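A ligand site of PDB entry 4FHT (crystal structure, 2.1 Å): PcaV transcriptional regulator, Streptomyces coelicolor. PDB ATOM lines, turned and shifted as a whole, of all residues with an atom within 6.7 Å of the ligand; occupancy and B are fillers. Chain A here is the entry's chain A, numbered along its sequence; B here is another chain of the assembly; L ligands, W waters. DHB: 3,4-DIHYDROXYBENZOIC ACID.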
ATOM      1  N   VAL A   7      -9.332 -16.538 -22.997  1.00  0.00           N
ATOM      2  CA  VAL A   7     -10.406 -17.351 -22.438  1.00  0.00           C
ATOM      3  C   VAL A   7     -11.739 -16.607 -22.506  1.00  0.00           C
ATOM      4  O   VAL A   7     -11.769 -15.381 -22.610  1.00  0.00           O
ATOM      5  CB  VAL A   7     -10.115 -17.740 -20.972  1.00  0.00           C
ATOM      6  CG1 VAL A   7      -8.863 -18.601 -20.886  1.00  0.00           C
ATOM      7  CG2 VAL A   7      -9.978 -16.503 -20.102  1.00  0.00           C
ATOM      8  N   LEU A   9     -14.578 -15.225 -20.600  1.00  0.00           N
ATOM      9  CA  LEU A   9     -14.850 -14.833 -19.224  1.00  0.00           C
ATOM     10  C   LEU A   9     -16.265 -15.188 -18.766  1.00  0.00           C
ATOM     11  O   LEU A   9     -16.535 -15.202 -17.562  1.00  0.00           O
ATOM     12  CB  LEU A   9     -14.608 -13.333 -19.027  1.00  0.00           C
ATOM     13  CG  LEU A   9     -13.164 -12.852 -19.174  1.00  0.00           C
ATOM     14  CD1 LEU A   9     -13.046 -11.392 -18.754  1.00  0.00           C
ATOM     15  CD2 LEU A   9     -12.224 -13.728 -18.368  1.00  0.00           C
ATOM     16  N   HIS A  12     -16.169 -18.052 -16.445  1.00  0.00           N
ATOM     17  CA  HIS A  12     -15.337 -17.889 -15.254  1.00  0.00           C
ATOM     18  C   HIS A  12     -16.164 -17.386 -14.068  1.00  0.00           C
ATOM     19  O   HIS A  12     -16.594 -16.237 -14.064  1.00  0.00           O
ATOM     20  CB  HIS A  12     -14.176 -16.934 -15.531  1.00  0.00           C
ATOM     21  CG  HIS A  12     -13.072 -17.548 -16.333  1.00  0.00           C
ATOM     22  ND1 HIS A  12     -11.744 -17.452 -15.968  1.00  0.00           N
ATOM     23  CD2 HIS A  12     -13.097 -18.288 -17.473  1.00  0.00           C
ATOM     24  CE1 HIS A  12     -11.000 -18.099 -16.847  1.00  0.00           C
ATOM     25  NE2 HIS A  12     -11.795 -18.610 -17.767  1.00  0.00           N
ATOM     26  N   PRO A  13     -16.353 -18.241 -13.060  1.00  0.00           N
ATOM     27  CA  PRO A  13     -17.224 -17.922 -11.912  1.00  0.00           C
ATOM     28  C   PRO A  13     -16.764 -16.669 -11.171  1.00  0.00           C
ATOM     29  O   PRO A  13     -17.593 -15.895 -10.687  1.00  0.00           O
ATOM     30  CB  PRO A  13     -17.096 -19.162 -11.020  1.00  0.00           C
ATOM     31  CG  PRO A  13     -15.820 -19.816 -11.451  1.00  0.00           C
ATOM     32  CD  PRO A  13     -15.715 -19.561 -12.908  1.00  0.00           C
ATOM     33  N   GLY A  14     -15.443 -16.467 -11.083  1.00  0.00           N
ATOM     34  CA  GLY A  14     -14.893 -15.294 -10.437  1.00  0.00           C
ATOM     35  C   GLY A  14     -15.209 -14.010 -11.188  1.00  0.00           C
ATOM     36  O   GLY A  14     -15.431 -12.961 -10.579  1.00  0.00           O
ATOM     37  N   HIS A  15     -15.243 -14.093 -12.513  1.00  0.00           N
ATOM     38  CA  HIS A  15     -15.599 -12.944 -13.337  1.00  0.00           C
ATOM     39  C   HIS A  15     -17.040 -12.544 -13.081  1.00  0.00           C
ATOM     40  O   HIS A  15     -17.348 -11.369 -12.890  1.00  0.00           O
ATOM     41  CB  HIS A  15     -15.391 -13.254 -14.817  1.00  0.00           C
ATOM     42  CG  HIS A  15     -15.812 -12.143 -15.734  1.00  0.00           C
ATOM     43  ND1 HIS A  15     -15.135 -10.944 -15.816  1.00  0.00           N
ATOM     44  CD2 HIS A  15     -16.843 -12.055 -16.609  1.00  0.00           C
ATOM     45  CE1 HIS A  15     -15.730 -10.169 -16.695  1.00  0.00           C
ATOM     46  NE2 HIS A  15     -16.774 -10.821 -17.188  1.00  0.00           N
ATOM     47  N   LEU A  16     -17.927 -13.537 -13.083  1.00  0.00           N
ATOM     48  CA  LEU A  16     -19.334 -13.314 -12.795  1.00  0.00           C
ATOM     49  C   LEU A  16     -19.537 -12.837 -11.361  1.00  0.00           C
ATOM     50  O   LEU A  16     -20.403 -12.001 -11.088  1.00  0.00           O
ATOM     51  CB  LEU A  16     -20.157 -14.582 -13.062  1.00  0.00           C
ATOM     52  CG  LEU A  16     -20.538 -14.931 -14.502  1.00  0.00           C
ATOM     53  CD1 LEU A  16     -20.985 -13.685 -15.256  1.00  0.00           C
ATOM     54  CD2 LEU A  16     -19.406 -15.621 -15.241  1.00  0.00           C
ATOM     55  N   ARG A  18     -17.456 -11.042  -9.439  1.00  0.00           N
ATOM     56  CA  ARG A  18     -17.087  -9.641  -9.318  1.00  0.00           C
ATOM     57  C   ARG A  18     -18.181  -8.731  -9.866  1.00  0.00           C
ATOM     58  O   ARG A  18     -18.547  -7.739  -9.230  1.00  0.00           O
ATOM     59  CB  ARG A  18     -15.766  -9.338 -10.047  1.00  0.00           C
ATOM     60  CG  ARG A  18     -15.515  -7.837 -10.178  1.00  0.00           C
ATOM     61  CD  ARG A  18     -14.158  -7.503 -10.773  1.00  0.00           C
ATOM     62  NE  ARG A  18     -14.020  -7.895 -12.167  1.00  0.00           N
ATOM     63  CZ  ARG A  18     -14.563  -7.254 -13.198  1.00  0.00           C
ATOM     64  NH1 ARG A  18     -15.306  -6.173 -12.989  1.00  0.00           N
ATOM     65  NH2 ARG A  18     -14.377  -7.693 -14.432  1.00  0.00           N
ATOM     66  N   ARG A  19     -18.712  -9.075 -11.033  1.00  0.00           N
ATOM     67  CA  ARG A  19     -19.712  -8.256 -11.684  1.00  0.00           C
ATOM     68  C   ARG A  19     -21.041  -8.253 -10.908  1.00  0.00           C
ATOM     69  O   ARG A  19     -21.736  -7.238 -10.871  1.00  0.00           O
ATOM     70  CB  ARG A  19     -19.911  -8.679 -13.133  1.00  0.00           C
ATOM     71  CG  ARG A  19     -18.645  -8.575 -13.969  1.00  0.00           C
ATOM     72  CD  ARG A  19     -18.883  -8.868 -15.437  1.00  0.00           C
ATOM     73  NE  ARG A  19     -19.736  -7.857 -16.059  1.00  0.00           N
ATOM     74  CZ  ARG A  19     -19.838  -7.678 -17.374  1.00  0.00           C
ATOM     75  NH1 ARG A  19     -19.135  -8.430 -18.206  1.00  0.00           N
ATOM     76  NH2 ARG A  19     -20.648  -6.745 -17.847  1.00  0.00           N
ATOM     77  N   HIS B  24     -14.449 -15.733  -3.892  1.00  0.00           N
ATOM     78  CA  HIS B  24     -13.638 -15.503  -5.086  1.00  0.00           C
ATOM     79  C   HIS B  24     -12.299 -14.877  -4.730  1.00  0.00           C
ATOM     80  O   HIS B  24     -11.235 -15.357  -5.143  1.00  0.00           O
ATOM     81  CB  HIS B  24     -14.395 -14.583  -6.053  1.00  0.00           C
ATOM     82  CG  HIS B  24     -13.587 -14.174  -7.253  1.00  0.00           C
ATOM     83  ND1 HIS B  24     -13.770 -12.961  -7.880  1.00  0.00           N
ATOM     84  CD2 HIS B  24     -12.622 -14.817  -7.940  1.00  0.00           C
ATOM     85  CE1 HIS B  24     -12.935 -12.878  -8.905  1.00  0.00           C
ATOM     86  NE2 HIS B  24     -12.228 -13.986  -8.962  1.00  0.00           N
ATOM     87  N   TRP B  28      -8.688 -16.573  -5.263  1.00  0.00           N
ATOM     88  CA  TRP B  28      -7.787 -15.901  -6.200  1.00  0.00           C
ATOM     89  C   TRP B  28      -6.419 -15.672  -5.551  1.00  0.00           C
ATOM     90  O   TRP B  28      -5.389 -16.033  -6.112  1.00  0.00           O
ATOM     91  CB  TRP B  28      -8.386 -14.570  -6.678  1.00  0.00           C
ATOM     92  CG  TRP B  28      -7.518 -13.862  -7.666  1.00  0.00           C
ATOM     93  CD1 TRP B  28      -6.512 -12.987  -7.389  1.00  0.00           C
ATOM     94  CD2 TRP B  28      -7.569 -13.964  -9.098  1.00  0.00           C
ATOM     95  NE1 TRP B  28      -5.931 -12.542  -8.554  1.00  0.00           N
ATOM     96  CE2 TRP B  28      -6.560 -13.127  -9.612  1.00  0.00           C
ATOM     97  CE3 TRP B  28      -8.370 -14.693  -9.990  1.00  0.00           C
ATOM     98  CZ2 TRP B  28      -6.338 -12.996 -10.981  1.00  0.00           C
ATOM     99  CZ3 TRP B  28      -8.143 -14.561 -11.347  1.00  0.00           C
ATOM    100  CH2 TRP B  28      -7.133 -13.712 -11.840  1.00  0.00           C
ATOM    101  N   VAL B  32      -4.148 -18.276  -7.278  1.00  0.00           N
ATOM    102  CA  VAL B  32      -3.775 -17.593  -8.506  1.00  0.00           C
ATOM    103  C   VAL B  32      -2.606 -16.618  -8.327  1.00  0.00           C
ATOM    104  O   VAL B  32      -1.504 -16.864  -8.811  1.00  0.00           O
ATOM    105  CB  VAL B  32      -4.965 -16.882  -9.169  1.00  0.00           C
ATOM    106  CG1 VAL B  32      -4.560 -16.269 -10.508  1.00  0.00           C
ATOM    107  CG2 VAL B  32      -6.121 -17.858  -9.352  1.00  0.00           C
ATOM    108  N   THR B  37      -4.307  -8.721  -9.763  1.00  0.00           N
ATOM    109  CA  THR B  37      -5.708  -8.853  -9.396  1.00  0.00           C
ATOM    110  C   THR B  37      -6.515  -9.444 -10.547  1.00  0.00           C
ATOM    111  O   THR B  37      -6.056  -9.486 -11.680  1.00  0.00           O
ATOM    112  CB  THR B  37      -6.326  -7.497  -8.999  1.00  0.00           C
ATOM    113  OG1 THR B  37      -6.391  -6.651 -10.147  1.00  0.00           O
ATOM    114  CG2 THR B  37      -5.497  -6.820  -7.901  1.00  0.00           C
ATOM    115  N   SER B  38      -7.725  -9.894 -10.239  1.00  0.00           N
ATOM    116  CA  SER B  38      -8.608 -10.434 -11.276  1.00  0.00           C
ATOM    117  C   SER B  38      -9.118  -9.390 -12.284  1.00  0.00           C
ATOM    118  O   SER B  38      -9.269  -9.720 -13.464  1.00  0.00           O
ATOM    119  CB  SER B  38      -9.766 -11.240 -10.656  1.00  0.00           C
ATOM    120  OG  SER B  38     -10.862 -10.422 -10.289  1.00  0.00           O
ATOM    121  N   PRO B  39      -9.379  -8.145 -11.844  1.00  0.00           N
ATOM    122  CA  PRO B  39      -9.657  -7.135 -12.873  1.00  0.00           C
ATOM    123  C   PRO B  39      -8.468  -6.909 -13.813  1.00  0.00           C
ATOM    124  O   PRO B  39      -8.660  -6.688 -15.007  1.00  0.00           O
ATOM    125  CB  PRO B  39      -9.937  -5.868 -12.057  1.00  0.00           C
ATOM    126  CG  PRO B  39     -10.467  -6.383 -10.763  1.00  0.00           C
ATOM    127  CD  PRO B  39      -9.686  -7.634 -10.495  1.00  0.00           C
ATOM    128  N   GLN B  40      -7.263  -6.977 -13.268  1.00  0.00           N
ATOM    129  CA  GLN B  40      -6.054  -6.811 -14.081  1.00  0.00           C
ATOM    130  C   GLN B  40      -5.925  -7.934 -15.103  1.00  0.00           C
ATOM    131  O   GLN B  40      -5.574  -7.686 -16.257  1.00  0.00           O
ATOM    132  CB  GLN B  40      -4.806  -6.749 -13.185  1.00  0.00           C
ATOM    133  CG  GLN B  40      -4.640  -5.414 -12.455  1.00  0.00           C
ATOM    134  CD  GLN B  40      -3.563  -5.475 -11.373  1.00  0.00           C
ATOM    135  OE1 GLN B  40      -2.809  -6.440 -11.277  1.00  0.00           O
ATOM    136  NE2 GLN B  40      -3.493  -4.423 -10.562  1.00  0.00           N
ATOM    137  N   TYR B  41      -6.213  -9.170 -14.693  1.00  0.00           N
ATOM    138  CA  TYR B  41      -6.179 -10.302 -15.603  1.00  0.00           C
ATOM    139  C   TYR B  41      -7.216 -10.163 -16.707  1.00  0.00           C
ATOM    140  O   TYR B  41      -6.945 -10.477 -17.869  1.00  0.00           O
ATOM    141  CB  TYR B  41      -6.375 -11.632 -14.864  1.00  0.00           C
ATOM    142  CG  TYR B  41      -6.495 -12.796 -15.821  1.00  0.00           C
ATOM    143  CD1 TYR B  41      -5.369 -13.444 -16.311  1.00  0.00           C
ATOM    144  CD2 TYR B  41      -7.745 -13.241 -16.262  1.00  0.00           C
ATOM    145  CE1 TYR B  41      -5.481 -14.512 -17.195  1.00  0.00           C
ATOM    146  CE2 TYR B  41      -7.870 -14.298 -17.143  1.00  0.00           C
ATOM    147  CZ  TYR B  41      -6.725 -14.924 -17.604  1.00  0.00           C
ATOM    148  OH  TYR B  41      -6.850 -15.981 -18.484  1.00  0.00           O
ATOM    149  N   ALA B  42      -8.406  -9.695 -16.329  1.00  0.00           N
ATOM    150  CA  ALA B  42      -9.504  -9.532 -17.276  1.00  0.00           C
ATOM    151  C   ALA B  42      -9.111  -8.569 -18.398  1.00  0.00           C
ATOM    152  O   ALA B  42      -9.438  -8.785 -19.560  1.00  0.00           O
ATOM    153  CB  ALA B  42     -10.748  -9.025 -16.573  1.00  0.00           C
ATOM    154  N   VAL B  43      -8.400  -7.511 -18.020  1.00  0.00           N
ATOM    155  CA  VAL B  43      -7.925  -6.526 -18.985  1.00  0.00           C
ATOM    156  C   VAL B  43      -6.864  -7.158 -19.883  1.00  0.00           C
ATOM    157  O   VAL B  43      -6.897  -7.011 -21.107  1.00  0.00           O
ATOM    158  CB  VAL B  43      -7.368  -5.278 -18.286  1.00  0.00           C
ATOM    159  CG1 VAL B  43      -6.685  -4.359 -19.292  1.00  0.00           C
ATOM    160  CG2 VAL B  43      -8.487  -4.560 -17.555  1.00  0.00           C
ATOM    161  N   VAL B  62     -15.113  -5.864 -20.022  1.00  0.00           N
ATOM    162  CA  VAL B  62     -14.856  -6.615 -18.793  1.00  0.00           C
ATOM    163  C   VAL B  62     -15.679  -6.141 -17.593  1.00  0.00           C
ATOM    164  O   VAL B  62     -15.553  -6.681 -16.500  1.00  0.00           O
ATOM    165  CB  VAL B  62     -13.365  -6.602 -18.421  1.00  0.00           C
ATOM    166  CG1 VAL B  62     -12.533  -7.210 -19.539  1.00  0.00           C
ATOM    167  CG2 VAL B  62     -12.906  -5.178 -18.139  1.00  0.00           C
ATOM    168  N   ILE B 113      -5.590 -20.284 -12.879  1.00  0.00           N
ATOM    169  CA  ILE B 113      -7.013 -19.965 -12.872  1.00  0.00           C
ATOM    170  C   ILE B 113      -7.875 -21.203 -13.150  1.00  0.00           C
ATOM    171  O   ILE B 113      -8.935 -21.389 -12.541  1.00  0.00           O
ATOM    172  CB  ILE B 113      -7.339 -18.855 -13.900  1.00  0.00           C
ATOM    173  CG1 ILE B 113      -6.738 -17.518 -13.444  1.00  0.00           C
ATOM    174  CG2 ILE B 113      -8.841 -18.702 -14.093  1.00  0.00           C
ATOM    175  CD1 ILE B 113      -6.911 -16.397 -14.446  1.00  0.00           C
ATOM    176  N   MET B 116      -8.163 -23.111 -10.033  1.00  0.00           N
ATOM    177  CA  MET B 116      -9.039 -22.399  -9.111  1.00  0.00           C
ATOM    178  C   MET B 116     -10.503 -22.632  -9.461  1.00  0.00           C
ATOM    179  O   MET B 116     -11.331 -22.868  -8.585  1.00  0.00           O
ATOM    180  CB  MET B 116      -8.749 -20.897  -9.113  1.00  0.00           C
ATOM    181  CG  MET B 116      -9.669 -20.104  -8.197  1.00  0.00           C
ATOM    182  SD  MET B 116      -9.667 -18.307  -8.427  1.00  0.00           S
ATOM    183  CE  MET B 116     -10.321 -18.181 -10.093  1.00  0.00           C
ATOM    184  N   ASN B 117     -10.811 -22.578 -10.749  1.00  0.00           N
ATOM    185  CA  ASN B 117     -12.179 -22.781 -11.212  1.00  0.00           C
ATOM    186  C   ASN B 117     -12.711 -24.188 -10.955  1.00  0.00           C
ATOM    187  O   ASN B 117     -13.902 -24.375 -10.729  1.00  0.00           O
ATOM    188  CB  ASN B 117     -12.323 -22.404 -12.686  1.00  0.00           C
ATOM    189  CG  ASN B 117     -12.294 -20.898 -12.910  1.00  0.00           C
ATOM    190  OD1 ASN B 117     -12.412 -20.122 -11.962  1.00  0.00           O
ATOM    191  ND2 ASN B 117     -12.135 -20.485 -14.158  1.00  0.00           N
ATOM    192  N   PHE B 120     -13.564 -24.022  -7.383  1.00  0.00           N
ATOM    193  CA  PHE B 120     -14.669 -23.091  -7.219  1.00  0.00           C
ATOM    194  C   PHE B 120     -16.010 -23.693  -7.644  1.00  0.00           C
ATOM    195  O   PHE B 120     -17.026 -23.494  -6.984  1.00  0.00           O
ATOM    196  CB  PHE B 120     -14.404 -21.797  -8.010  1.00  0.00           C
ATOM    197  CG  PHE B 120     -14.991 -20.562  -7.389  1.00  0.00           C
ATOM    198  CD1 PHE B 120     -15.842 -20.650  -6.305  1.00  0.00           C
ATOM    199  CD2 PHE B 120     -14.700 -19.305  -7.900  1.00  0.00           C
ATOM    200  CE1 PHE B 120     -16.391 -19.510  -5.735  1.00  0.00           C
ATOM    201  CE2 PHE B 120     -15.241 -18.167  -7.348  1.00  0.00           C
ATOM    202  CZ  PHE B 120     -16.093 -18.264  -6.263  1.00  0.00           C
HETATM  203  C1  DHB L   1     -12.121 -12.131 -13.541  1.00  0.00           C
HETATM  204  C2  DHB L   1     -12.123 -12.948 -12.416  1.00  0.00           C
HETATM  205  C3  DHB L   1     -11.733 -14.266 -12.513  1.00  0.00           C
HETATM  206  O3  DHB L   1     -11.727 -15.085 -11.406  1.00  0.00           O
HETATM  207  C4  DHB L   1     -11.338 -14.788 -13.742  1.00  0.00           C
HETATM  208  O4  DHB L   1     -10.934 -16.104 -13.822  1.00  0.00           O
HETATM  209  C5  DHB L   1     -11.335 -13.981 -14.866  1.00  0.00           C
HETATM  210  C6  DHB L   1     -11.729 -12.642 -14.762  1.00  0.00           C
HETATM  211  C   DHB L   1     -12.549 -10.702 -13.440  1.00  0.00           C
HETATM  212  O1  DHB L   1     -12.392 -10.059 -12.363  1.00  0.00           O
HETATM  213  O2  DHB L   1     -13.061 -10.129 -14.439  1.00  0.00           O
HETATM  214  O   HOH W   1     -13.143 -17.567 -12.226  1.00  0.00           O
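Water W1 lies within hydrogen-bond range of the side-chain amide oxygen (OD1) of Asn 117 of chain B (2.7 Å), the backbone NH (N) of Gly 14 (2.8 Å) and an oxygen (O3) of the ligand (3.0 Å).
Merely in contact with the ligand: Leu 9 (3.6 Å), Gly 14 (3.3 Å), Trp 28 of chain B (3.6 Å), Pro 39 of chain B (3.6 Å), Tyr 41 of chain B (3.9 Å), Ala 42 of chain B (3.3 Å), Ile 113 of chain B (3.3 Å) and Met 116 of chain B (3.6 Å).
Hydrophobic or aromatic side chains that line the ligand: Leu 9, His 12, His 15, His 24 of chain B, Trp 28 of chain B, Tyr 41 of chain B, Ala 42 of chain B, Ile 113 of chain B and Met 116 of chain B.
13 residues have an atom within 4 Å of the ligand: Leu 9, His 12, Gly 14, His 15, Arg 18, His 24 of chain B, Trp 28 of chain B, Ser 38 of chain B, Pro 39 of chain B, Tyr 41 of chain B, Ala 42 of chain B, Ile 113 of chain B and Met 116 of chain B.
The nearest printed residue that does not touch the ligand is Asn 117 of chain B (4.6 Å).
The backbone carbonyl oxygen of Val 62 of chain B is in hydrogen-bond range of the guanidinium group of Arg 18 (2.6 Å).
O of Gly 14 sits close to ND1 of His 24 of chain B (3.2 Å).
N of Trp 28 of chain B sits at hydrogen-bond distance from SD of Met 116 of chain B, 3.7 Å away.
O1 of the ligand is in hydrogen-bond range of OG of Ser 38 of chain B (2.6 Å).
A ring nitrogen (ND1) of His 15 is in hydrogen-bond range of an oxygen (O2) of the ligand.
An oxygen (O4) of the ligand sits at hydrogen-bond distance from a ring nitrogen (ND1) of His 12.
An oxygen (O1) of the ligand lies within salt-bridge range of the guanidinium group (NE) of Arg 18, 2.7 Å away.
An oxygen (O3) of the ligand sits at hydrogen-bond distance from a ring nitrogen (NE2) of His 24 of chain B (2.7 Å).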
